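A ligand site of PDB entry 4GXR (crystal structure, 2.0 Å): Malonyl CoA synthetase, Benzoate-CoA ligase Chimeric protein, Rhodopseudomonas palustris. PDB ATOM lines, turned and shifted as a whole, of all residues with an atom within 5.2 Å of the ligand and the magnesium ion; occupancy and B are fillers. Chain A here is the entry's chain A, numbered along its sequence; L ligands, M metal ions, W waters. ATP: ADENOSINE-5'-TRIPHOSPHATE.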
ATOM      1  N   THR A 163      -5.770 -34.100 -28.762  1.00  0.00           N
ATOM      2  CA  THR A 163      -5.039 -33.258 -27.828  1.00  0.00           C
ATOM      3  C   THR A 163      -3.596 -33.083 -28.317  1.00  0.00           C
ATOM      4  O   THR A 163      -3.145 -33.810 -29.201  1.00  0.00           O
ATOM      5  CB  THR A 163      -5.053 -33.871 -26.419  1.00  0.00           C
ATOM      6  OG1 THR A 163      -4.447 -35.173 -26.465  1.00  0.00           O
ATOM      7  CG2 THR A 163      -6.490 -33.980 -25.906  1.00  0.00           C
ATOM      8  N   SER A 164      -2.873 -32.118 -27.748  1.00  0.00           N
ATOM      9  CA  SER A 164      -1.563 -31.749 -28.300  1.00  0.00           C
ATOM     10  C   SER A 164      -0.473 -32.798 -28.071  1.00  0.00           C
ATOM     11  O   SER A 164       0.548 -32.795 -28.746  1.00  0.00           O
ATOM     12  CB  SER A 164      -1.127 -30.381 -27.786  1.00  0.00           C
ATOM     13  OG  SER A 164      -2.027 -29.375 -28.240  1.00  0.00           O
ATOM     14  N   GLY A 165      -0.698 -33.701 -27.115  1.00  0.00           N
ATOM     15  CA  GLY A 165       0.246 -34.779 -26.812  1.00  0.00           C
ATOM     16  C   GLY A 165       1.302 -34.421 -25.788  1.00  0.00           C
ATOM     17  O   GLY A 165       2.325 -35.102 -25.684  1.00  0.00           O
ATOM     18  N   THR A 166       1.064 -33.370 -25.008  1.00  0.00           N
ATOM     19  CA  THR A 166       2.065 -32.867 -24.051  1.00  0.00           C
ATOM     20  C   THR A 166       2.358 -33.851 -22.916  1.00  0.00           C
ATOM     21  O   THR A 166       3.522 -33.967 -22.498  1.00  0.00           O
ATOM     22  CB  THR A 166       1.631 -31.509 -23.447  1.00  0.00           C
ATOM     23  OG1 THR A 166       1.435 -30.562 -24.501  1.00  0.00           O
ATOM     24  CG2 THR A 166       2.688 -30.976 -22.481  1.00  0.00           C
ATOM     25  N   THR A 167       1.346 -34.542 -22.411  1.00  0.00           N
ATOM     26  CA  THR A 167       1.514 -35.433 -21.253  1.00  0.00           C
ATOM     27  C   THR A 167       1.576 -36.906 -21.646  1.00  0.00           C
ATOM     28  O   THR A 167       1.810 -37.753 -20.793  1.00  0.00           O
ATOM     29  CB  THR A 167       0.377 -35.250 -20.235  1.00  0.00           C
ATOM     30  OG1 THR A 167      -0.867 -35.686 -20.809  1.00  0.00           O
ATOM     31  CG2 THR A 167       0.277 -33.795 -19.813  1.00  0.00           C
ATOM     32  N   GLY A 168       1.362 -37.202 -22.925  1.00  0.00           N
ATOM     33  CA  GLY A 168       1.330 -38.571 -23.421  1.00  0.00           C
ATOM     34  C   GLY A 168       0.776 -38.577 -24.827  1.00  0.00           C
ATOM     35  O   GLY A 168       0.564 -37.520 -25.423  1.00  0.00           O
ATOM     36  N   ARG A 169       0.524 -39.767 -25.366  1.00  0.00           N
ATOM     37  CA  ARG A 169       0.000 -39.892 -26.726  1.00  0.00           C
ATOM     38  C   ARG A 169      -1.329 -39.151 -26.846  1.00  0.00           C
ATOM     39  O   ARG A 169      -2.220 -39.305 -26.009  1.00  0.00           O
ATOM     40  CB  ARG A 169      -0.195 -41.363 -27.082  1.00  0.00           C
ATOM     41  CG  ARG A 169      -0.565 -41.605 -28.546  1.00  0.00           C
ATOM     42  CD  ARG A 169      -0.524 -43.090 -28.859  1.00  0.00           C
ATOM     43  NE  ARG A 169      -1.466 -43.832 -28.022  1.00  0.00           N
ATOM     44  CZ  ARG A 169      -1.460 -45.159 -27.854  1.00  0.00           C
ATOM     45  NH1 ARG A 169      -2.383 -45.711 -27.068  1.00  0.00           N
ATOM     46  NH2 ARG A 169      -0.565 -45.930 -28.465  1.00  0.00           N
ATOM     47  N   SER A 170      -1.464 -38.340 -27.900  1.00  0.00           N
ATOM     48  CA  SER A 170      -2.683 -37.558 -28.128  1.00  0.00           C
ATOM     49  C   SER A 170      -3.943 -38.425 -28.086  1.00  0.00           C
ATOM     50  O   SER A 170      -3.943 -39.537 -28.615  1.00  0.00           O
ATOM     51  CB  SER A 170      -2.586 -36.863 -29.486  1.00  0.00           C
ATOM     52  OG  SER A 170      -1.491 -35.962 -29.504  1.00  0.00           O
ATOM     53  N   MLY A 171      -4.998 -37.901 -27.458  1.00  0.00           N
ATOM     54  CA  MLY A 171      -6.311 -38.556 -27.388  1.00  0.00           C
ATOM     55  CB  MLY A 171      -6.814 -38.553 -25.943  1.00  0.00           C
ATOM     56  CG  MLY A 171      -5.818 -39.131 -24.945  1.00  0.00           C
ATOM     57  CD  MLY A 171      -6.434 -39.184 -23.546  1.00  0.00           C
ATOM     58  CE  MLY A 171      -5.509 -38.701 -22.422  1.00  0.00           C
ATOM     59  NZ  MLY A 171      -4.919 -37.368 -22.648  1.00  0.00           N
ATOM     60  CH1 MLY A 171      -5.945 -36.334 -22.826  1.00  0.00           C
ATOM     61  CH2 MLY A 171      -4.122 -37.008 -21.470  1.00  0.00           C
ATOM     62  C   MLY A 171      -7.331 -37.802 -28.202  1.00  0.00           C
ATOM     63  O   MLY A 171      -7.306 -36.574 -28.227  1.00  0.00           O
ATOM     64  N   HIS A 207      -5.599 -26.872 -34.248  1.00  0.00           N
ATOM     65  CA  HIS A 207      -5.738 -26.735 -32.793  1.00  0.00           C
ATOM     66  C   HIS A 207      -7.011 -25.942 -32.510  1.00  0.00           C
ATOM     67  O   HIS A 207      -7.416 -25.097 -33.308  1.00  0.00           O
ATOM     68  CB  HIS A 207      -4.502 -26.031 -32.232  1.00  0.00           C
ATOM     69  CG  HIS A 207      -4.485 -25.914 -30.734  1.00  0.00           C
ATOM     70  ND1 HIS A 207      -5.011 -24.840 -30.065  1.00  0.00           N
ATOM     71  CD2 HIS A 207      -3.967 -26.734 -29.777  1.00  0.00           C
ATOM     72  CE1 HIS A 207      -4.852 -24.994 -28.767  1.00  0.00           C
ATOM     73  NE2 HIS A 207      -4.220 -26.140 -28.565  1.00  0.00           N
ATOM     74  N   GLY A 276      -4.018 -17.062 -25.197  1.00  0.00           N
ATOM     75  CA  GLY A 276      -4.516 -18.373 -24.777  1.00  0.00           C
ATOM     76  C   GLY A 276      -3.526 -19.494 -25.033  1.00  0.00           C
ATOM     77  O   GLY A 276      -2.449 -19.263 -25.574  1.00  0.00           O
ATOM     78  N   SER A 277      -3.914 -20.715 -24.635  1.00  0.00           N
ATOM     79  CA  SER A 277      -3.280 -21.972 -25.042  1.00  0.00           C
ATOM     80  C   SER A 277      -2.042 -22.364 -24.227  1.00  0.00           C
ATOM     81  O   SER A 277      -1.594 -23.496 -24.323  1.00  0.00           O
ATOM     82  CB  SER A 277      -2.933 -21.985 -26.538  1.00  0.00           C
ATOM     83  OG  SER A 277      -4.058 -21.608 -27.324  1.00  0.00           O
ATOM     84  N   ALA A 278      -1.488 -21.421 -23.472  1.00  0.00           N
ATOM     85  CA  ALA A 278      -0.376 -21.664 -22.560  1.00  0.00           C
ATOM     86  C   ALA A 278      -0.376 -20.518 -21.544  1.00  0.00           C
ATOM     87  O   ALA A 278      -1.049 -19.512 -21.768  1.00  0.00           O
ATOM     88  CB  ALA A 278       0.946 -21.729 -23.318  1.00  0.00           C
ATOM     89  N   PRO A 279       0.370 -20.648 -20.429  1.00  0.00           N
ATOM     90  CA  PRO A 279       0.289 -19.584 -19.417  1.00  0.00           C
ATOM     91  C   PRO A 279       0.893 -18.266 -19.899  1.00  0.00           C
ATOM     92  O   PRO A 279       2.020 -18.249 -20.368  1.00  0.00           O
ATOM     93  CB  PRO A 279       1.097 -20.137 -18.227  1.00  0.00           C
ATOM     94  CG  PRO A 279       1.313 -21.584 -18.507  1.00  0.00           C
ATOM     95  CD  PRO A 279       1.170 -21.797 -19.986  1.00  0.00           C
ATOM     96  N   LEU A 280       0.134 -17.181 -19.807  1.00  0.00           N
ATOM     97  CA  LEU A 280       0.715 -15.859 -20.030  1.00  0.00           C
ATOM     98  C   LEU A 280       1.286 -15.393 -18.695  1.00  0.00           C
ATOM     99  O   LEU A 280       0.540 -15.144 -17.746  1.00  0.00           O
ATOM    100  CB  LEU A 280      -0.317 -14.850 -20.551  1.00  0.00           C
ATOM    101  CG  LEU A 280       0.229 -13.456 -20.883  1.00  0.00           C
ATOM    102  CD1 LEU A 280       1.074 -13.483 -22.144  1.00  0.00           C
ATOM    103  CD2 LEU A 280      -0.891 -12.441 -21.004  1.00  0.00           C
ATOM    104  N   GLU A 298      -6.524 -12.649 -21.174  1.00  0.00           N
ATOM    105  CA  GLU A 298      -6.211 -14.063 -21.190  1.00  0.00           C
ATOM    106  C   GLU A 298      -7.436 -14.916 -20.913  1.00  0.00           C
ATOM    107  O   GLU A 298      -8.262 -14.572 -20.056  1.00  0.00           O
ATOM    108  CB  GLU A 298      -5.118 -14.398 -20.174  1.00  0.00           C
ATOM    109  CG  GLU A 298      -4.660 -15.838 -20.221  1.00  0.00           C
ATOM    110  CD  GLU A 298      -3.484 -16.124 -19.296  1.00  0.00           C
ATOM    111  OE1 GLU A 298      -3.273 -15.330 -18.367  1.00  0.00           O
ATOM    112  OE2 GLU A 298      -2.789 -17.142 -19.500  1.00  0.00           O
ATOM    113  N   ARG A 299      -7.559 -16.022 -21.633  1.00  0.00           N
ATOM    114  CA  ARG A 299      -8.616 -17.004 -21.417  1.00  0.00           C
ATOM    115  C   ARG A 299      -8.035 -18.413 -21.397  1.00  0.00           C
ATOM    116  O   ARG A 299      -6.953 -18.664 -21.924  1.00  0.00           O
ATOM    117  CB  ARG A 299      -9.763 -16.843 -22.448  1.00  0.00           C
ATOM    118  CG  ARG A 299      -9.623 -17.634 -23.744  1.00  0.00           C
ATOM    119  CD  ARG A 299      -8.426 -17.185 -24.575  1.00  0.00           C
ATOM    120  NE  ARG A 299      -8.325 -17.926 -25.841  1.00  0.00           N
ATOM    121  CZ  ARG A 299      -7.878 -19.174 -25.954  1.00  0.00           C
ATOM    122  NH1 ARG A 299      -7.831 -19.758 -27.147  1.00  0.00           N
ATOM    123  NH2 ARG A 299      -7.490 -19.866 -24.879  1.00  0.00           N
ATOM    124  N   TYR A 300      -8.759 -19.329 -20.759  1.00  0.00           N
ATOM    125  CA  TYR A 300      -8.283 -20.703 -20.531  1.00  0.00           C
ATOM    126  C   TYR A 300      -9.258 -21.707 -21.098  1.00  0.00           C
ATOM    127  O   TYR A 300     -10.450 -21.695 -20.752  1.00  0.00           O
ATOM    128  CB  TYR A 300      -8.095 -20.943 -19.046  1.00  0.00           C
ATOM    129  CG  TYR A 300      -8.138 -22.381 -18.557  1.00  0.00           C
ATOM    130  CD1 TYR A 300      -7.203 -23.326 -18.990  1.00  0.00           C
ATOM    131  CD2 TYR A 300      -9.070 -22.785 -17.606  1.00  0.00           C
ATOM    132  CE1 TYR A 300      -7.223 -24.636 -18.518  1.00  0.00           C
ATOM    133  CE2 TYR A 300      -9.102 -24.084 -17.129  1.00  0.00           C
ATOM    134  CZ  TYR A 300      -8.185 -25.007 -17.576  1.00  0.00           C
ATOM    135  OH  TYR A 300      -8.228 -26.291 -17.076  1.00  0.00           O
ATOM    136  N   GLY A 301      -8.723 -22.573 -21.942  1.00  0.00           N
ATOM    137  CA  GLY A 301      -9.472 -23.677 -22.516  1.00  0.00           C
ATOM    138  C   GLY A 301      -8.599 -24.890 -22.742  1.00  0.00           C
ATOM    139  O   GLY A 301      -7.388 -24.874 -22.478  1.00  0.00           O
ATOM    140  N   MET A 302      -9.237 -25.963 -23.218  1.00  0.00           N
ATOM    141  CA  MET A 302      -8.564 -27.225 -23.539  1.00  0.00           C
ATOM    142  C   MET A 302      -9.257 -27.837 -24.731  1.00  0.00           C
ATOM    143  O   MET A 302     -10.421 -27.528 -25.010  1.00  0.00           O
ATOM    144  CB  MET A 302      -8.695 -28.250 -22.395  1.00  0.00           C
ATOM    145  CG  MET A 302      -8.417 -27.754 -20.995  1.00  0.00           C
ATOM    146  SD  MET A 302      -8.958 -28.956 -19.756  1.00  0.00           S
ATOM    147  CE  MET A 302      -8.245 -30.475 -20.355  1.00  0.00           C
ATOM    148  N   THR A 303      -8.568 -28.732 -25.417  1.00  0.00           N
ATOM    149  CA  THR A 303      -9.174 -29.481 -26.505  1.00  0.00           C
ATOM    150  C   THR A 303     -10.521 -30.094 -26.087  1.00  0.00           C
ATOM    151  O   THR A 303     -11.511 -29.978 -26.811  1.00  0.00           O
ATOM    152  CB  THR A 303      -8.219 -30.573 -27.016  1.00  0.00           C
ATOM    153  OG1 THR A 303      -7.014 -29.936 -27.491  1.00  0.00           O
ATOM    154  CG2 THR A 303      -8.857 -31.371 -28.152  1.00  0.00           C
ATOM    155  N   GLU A 304     -10.560 -30.707 -24.900  1.00  0.00           N
ATOM    156  CA  GLU A 304     -11.763 -31.412 -24.425  1.00  0.00           C
ATOM    157  C   GLU A 304     -12.915 -30.512 -23.968  1.00  0.00           C
ATOM    158  O   GLU A 304     -14.047 -30.986 -23.835  1.00  0.00           O
ATOM    159  CB  GLU A 304     -11.397 -32.327 -23.254  1.00  0.00           C
ATOM    160  CG  GLU A 304     -10.374 -33.411 -23.554  1.00  0.00           C
ATOM    161  CD  GLU A 304      -8.967 -33.024 -23.159  1.00  0.00           C
ATOM    162  OE1 GLU A 304      -8.580 -31.850 -23.391  1.00  0.00           O
ATOM    163  OE2 GLU A 304      -8.231 -33.883 -22.635  1.00  0.00           O
ATOM    164  N   VAL A 322      -6.584 -16.523 -15.214  1.00  0.00           N
ATOM    165  CA  VAL A 322      -7.298 -16.809 -16.463  1.00  0.00           C
ATOM    166  C   VAL A 322      -8.787 -16.429 -16.401  1.00  0.00           C
ATOM    167  O   VAL A 322      -9.551 -16.750 -17.324  1.00  0.00           O
ATOM    168  CB  VAL A 322      -7.110 -18.287 -16.900  1.00  0.00           C
ATOM    169  CG1 VAL A 322      -5.637 -18.529 -17.242  1.00  0.00           C
ATOM    170  CG2 VAL A 322      -7.577 -19.247 -15.818  1.00  0.00           C
ATOM    171  N   THR A 380      -9.976 -31.665 -15.228  1.00  0.00           N
ATOM    172  CA  THR A 380      -9.129 -31.043 -16.243  1.00  0.00           C
ATOM    173  C   THR A 380      -7.703 -31.577 -16.263  1.00  0.00           C
ATOM    174  O   THR A 380      -7.047 -31.552 -17.297  1.00  0.00           O
ATOM    175  CB  THR A 380      -9.017 -29.507 -16.078  1.00  0.00           C
ATOM    176  OG1 THR A 380      -8.365 -29.206 -14.833  1.00  0.00           O
ATOM    177  CG2 THR A 380     -10.380 -28.845 -16.136  1.00  0.00           C
ATOM    178  N   ASP A 382      -5.572 -29.983 -14.519  1.00  0.00           N
ATOM    179  CA  ASP A 382      -4.882 -28.757 -14.171  1.00  0.00           C
ATOM    180  C   ASP A 382      -5.124 -28.398 -12.710  1.00  0.00           C
ATOM    181  O   ASP A 382      -6.269 -28.435 -12.236  1.00  0.00           O
ATOM    182  CB  ASP A 382      -5.345 -27.613 -15.073  1.00  0.00           C
ATOM    183  CG  ASP A 382      -4.977 -27.835 -16.543  1.00  0.00           C
ATOM    184  OD1 ASP A 382      -3.873 -28.383 -16.795  1.00  0.00           O
ATOM    185  OD2 ASP A 382      -5.778 -27.475 -17.432  1.00  0.00           O
ATOM    186  N   ILE A 394      -4.325 -20.782 -12.576  1.00  0.00           N
ATOM    187  CA  ILE A 394      -3.745 -22.088 -12.859  1.00  0.00           C
ATOM    188  C   ILE A 394      -2.332 -22.134 -12.318  1.00  0.00           C
ATOM    189  O   ILE A 394      -1.478 -21.322 -12.679  1.00  0.00           O
ATOM    190  CB  ILE A 394      -3.793 -22.408 -14.369  1.00  0.00           C
ATOM    191  CG1 ILE A 394      -5.252 -22.519 -14.822  1.00  0.00           C
ATOM    192  CG2 ILE A 394      -3.040 -23.706 -14.673  1.00  0.00           C
ATOM    193  CD1 ILE A 394      -5.423 -22.608 -16.314  1.00  0.00           C
ATOM    194  N   ARG A 397       0.073 -28.072 -14.368  1.00  0.00           N
ATOM    195  CA  ARG A 397      -0.539 -29.356 -14.677  1.00  0.00           C
ATOM    196  C   ARG A 397      -0.315 -30.294 -13.515  1.00  0.00           C
ATOM    197  O   ARG A 397       0.747 -30.275 -12.888  1.00  0.00           O
ATOM    198  CB  ARG A 397       0.089 -29.977 -15.925  1.00  0.00           C
ATOM    199  CG  ARG A 397      -0.053 -29.185 -17.216  1.00  0.00           C
ATOM    200  CD  ARG A 397       0.700 -29.901 -18.324  1.00  0.00           C
ATOM    201  NE  ARG A 397       0.695 -29.187 -19.607  1.00  0.00           N
ATOM    202  CZ  ARG A 397      -0.206 -29.345 -20.575  1.00  0.00           C
ATOM    203  NH1 ARG A 397      -0.090 -28.641 -21.701  1.00  0.00           N
ATOM    204  NH2 ARG A 397      -1.209 -30.205 -20.448  1.00  0.00           N
HETATM  205  PG  ATP L   1      -2.426 -33.607 -23.845  1.00  0.00           P
HETATM  206  O1G ATP L   1      -3.823 -33.432 -23.305  1.00  0.00           O
HETATM  207  O2G ATP L   1      -1.384 -33.884 -22.764  1.00  0.00           O
HETATM  208  O3G ATP L   1      -2.378 -34.538 -25.023  1.00  0.00           O
HETATM  209  PB  ATP L   1      -2.351 -30.738 -23.941  1.00  0.00           P
HETATM  210  O1B ATP L   1      -3.089 -30.884 -22.624  1.00  0.00           O
HETATM  211  O2B ATP L   1      -1.195 -29.796 -24.046  1.00  0.00           O
HETATM  212  O3B ATP L   1      -1.920 -32.205 -24.457  1.00  0.00           O
HETATM  213  PA  ATP L   1      -4.231 -28.986 -25.257  1.00  0.00           P
HETATM  214  O1A ATP L   1      -5.689 -29.384 -25.141  1.00  0.00           O
HETATM  215  O2A ATP L   1      -3.784 -28.319 -26.543  1.00  0.00           O
HETATM  216  O3A ATP L   1      -3.407 -30.363 -25.101  1.00  0.00           O
HETATM  217  O5' ATP L   1      -3.812 -28.031 -24.047  1.00  0.00           O
HETATM  218  C5' ATP L   1      -4.671 -27.771 -22.934  1.00  0.00           C
HETATM  219  C4' ATP L   1      -3.816 -27.496 -21.700  1.00  0.00           C
HETATM  220  O4' ATP L   1      -2.941 -26.382 -21.900  1.00  0.00           O
HETATM  221  C3' ATP L   1      -4.622 -27.139 -20.460  1.00  0.00           C
HETATM  222  O3' ATP L   1      -5.188 -28.287 -19.832  1.00  0.00           O
HETATM  223  C2' ATP L   1      -3.593 -26.413 -19.623  1.00  0.00           C
HETATM  224  O2' ATP L   1      -2.757 -27.322 -18.899  1.00  0.00           O
HETATM  225  C1' ATP L   1      -2.791 -25.675 -20.671  1.00  0.00           C
HETATM  226  N9  ATP L   1      -3.294 -24.305 -20.856  1.00  0.00           N
HETATM  227  C8  ATP L   1      -4.072 -23.869 -21.865  1.00  0.00           C
HETATM  228  N7  ATP L   1      -4.353 -22.548 -21.718  1.00  0.00           N
HETATM  229  C5  ATP L   1      -3.750 -22.130 -20.600  1.00  0.00           C
HETATM  230  C6  ATP L   1      -3.639 -20.859 -19.864  1.00  0.00           C
HETATM  231  N6  ATP L   1      -4.238 -19.744 -20.323  1.00  0.00           N
HETATM  232  N1  ATP L   1      -2.911 -20.857 -18.735  1.00  0.00           N
HETATM  233  C2  ATP L   1      -2.302 -21.959 -18.261  1.00  0.00           C
HETATM  234  N3  ATP L   1      -2.364 -23.151 -18.878  1.00  0.00           N
HETATM  235  C4  ATP L   1      -3.055 -23.295 -20.035  1.00  0.00           C
HETATM  236 MG    MG M   1      -4.380 -32.101 -21.989  1.00  0.00          MG
HETATM  237  O   HOH W   1      -2.690 -37.246 -24.155  1.00  0.00           O
HETATM  238  O   HOH W   2      -2.190 -19.082 -16.596  1.00  0.00           O
HETATM  239  O   HOH W   3      -4.670 -30.777 -20.282  1.00  0.00           O
HETATM  240  O   HOH W   4      -2.965 -33.055 -20.533  1.00  0.00           O
HETATM  241  O   HOH W   5      -5.863 -33.355 -21.287  1.00  0.00           O
HETATM  242  O   HOH W   6      -1.000 -25.338 -17.471  1.00  0.00           O
HETATM  243  O   HOH W   7      -5.943 -31.209 -23.113  1.00  0.00           O
HETATM  244  O   HOH W   8      -0.848 -27.229 -24.823  1.00  0.00           O
HETATM  245  O   HOH W   9      -5.665 -25.136 -24.841  1.00  0.00           O
HETATM  246  O   HOH W  10      -2.989 -25.544 -25.751  1.00  0.00           O
HETATM  247  O   HOH W  11      -0.172 -25.304 -22.858  1.00  0.00           O
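O1B of the ligand is bound to the magnesium ion, 1.9 Å away.
The magnesium ion is bound by O1G of the ligand.
The magnesium ion is bound by water W5, at 2.1 Å.
Water W7 is bound to the magnesium ion (2.1 Å).
The magnesium ion is bound by water W3 (2.2 Å).
The magnesium ion is bound by water W4, at 2.2 Å.
The magnesium ion has six donor atoms within binding distance.
An oxygen (O1A) of the ligand lies within hydrogen-bond range of the backbone NH of Thr 303 (3.0 Å).
A ring nitrogen (NE2) of His 207 sits at hydrogen-bond distance from an oxygen (O2A) of the ligand, at 3.0 Å.
O2A of the ligand sits at hydrogen-bond distance from OG of Ser 164, at 2.7 Å.
The side-chain hydroxyl (OG1) of Thr 163 is in hydrogen-bond range of an oxygen (O3G) of the ligand, at 2.6 Å.
The backbone NH of Gly 165 sits at hydrogen-bond distance from an oxygen (O3G) of the ligand (2.8 Å).
An oxygen (O2B) of the ligand is in salt-bridge range of the guanidinium group (NH1) of Arg 397 (2.8 Å).
The backbone NH (N) of Thr 167 is in hydrogen-bond range of an oxygen (O2G) of the ligand, 2.8 Å away.
N of Thr 166 lies within hydrogen-bond range of O3B of the ligand, 3.3 Å away.
The backbone carbonyl oxygen (O) of Arg 299 is in hydrogen-bond range of a nitrogen (N6) of the ligand.
The backbone NH of Ser 164 sits at hydrogen-bond distance from an oxygen (O3A) of the ligand, at 3.2 Å.
N6 of the ligand sits at hydrogen-bond distance from OE2 of Glu 298 (3.1 Å).
OD2 of Asp 382 sits at hydrogen-bond distance from O3' of the ligand (2.6 Å).
N of Ser 277 lies close to N7 of the ligand (3.5 Å).
OG1 of Thr 166 lies within hydrogen-bond range of O2B of the ligand.
The side-chain hydroxyl (OG1) of Thr 167 sits at hydrogen-bond distance from an oxygen (O2G) of the ligand.
OG1 of Thr 303 is in hydrogen-bond range of O1A of the ligand, at 2.8 Å.
No residue comes within 4 Å of the magnesium ion.
The nearest printed residue that does not touch the magnesium ion is Arg 397 (4.003 Å).
Water W4 lies within hydrogen-bond range of O2G of the ligand, NH2 of Arg 397 and OG1 of Thr 167.
Water W7 bridges OE1 of Glu 304 and O1A of the ligand.
Water W1 lies within hydrogen-bond range of O of Arg 169 (2.8 Å) and O3G of the ligand (2.9 Å).
Water W10 lies within hydrogen-bond range of the backbone carbonyl oxygen of Ser 277 (2.9 Å), an oxygen (O2A) of the ligand (3.0 Å) and a ring nitrogen (NE2) of His 207 (3.1 Å).
Water W11 lies within hydrogen-bond range of the backbone carbonyl oxygen of Ser 277 (2.7 Å) and an oxygen (O4') of the ligand (3.1 Å).
Residues that only touch the ligand: MLY 171 (3.6 Å), Ala 278 (3.5 Å), Pro 279 (3.5 Å), Tyr 300 (3.99 Å), Gly 301 (3.5 Å), Met 302 (3.5 Å), Val 322 (3.6 Å) and Ile 394 (3.7 Å).
Hydrophobic or aromatic side chains within 4 Å of the ligand: His 207, Pro 279, Tyr 300, Met 302, Val 322 and Ile 394.
20 residues have an atom within 4 Å of the ligand: Thr 163, Ser 164, Gly 165, Thr 166, Thr 167, MLY 171, His 207, Ser 277, Ala 278, Pro 279, Glu 298, Arg 299, Tyr 300, Gly 301, Met 302, Thr 303, Val 322, Asp 382, Ile 394 and Arg 397.
The backbone NH of Leu 280 is in hydrogen-bond range of the side-chain carboxylate of Glu 298.
The backbone NH of Gly 165 is in hydrogen-bond range of the side-chain hydroxyl of Ser 170.
O of Thr 163 is in hydrogen-bond range of OG of Ser 170 (2.7 Å).
OH of Tyr 300 lies within hydrogen-bond range of OD2 of Asp 382 (2.7 Å).
N of Asp 382 is in hydrogen-bond range of OG1 of Thr 380 (2.9 Å).
The side-chain hydroxyl (OG1) of Thr 163 is in hydrogen-bond range of N of MLY 171 (3.0 Å).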
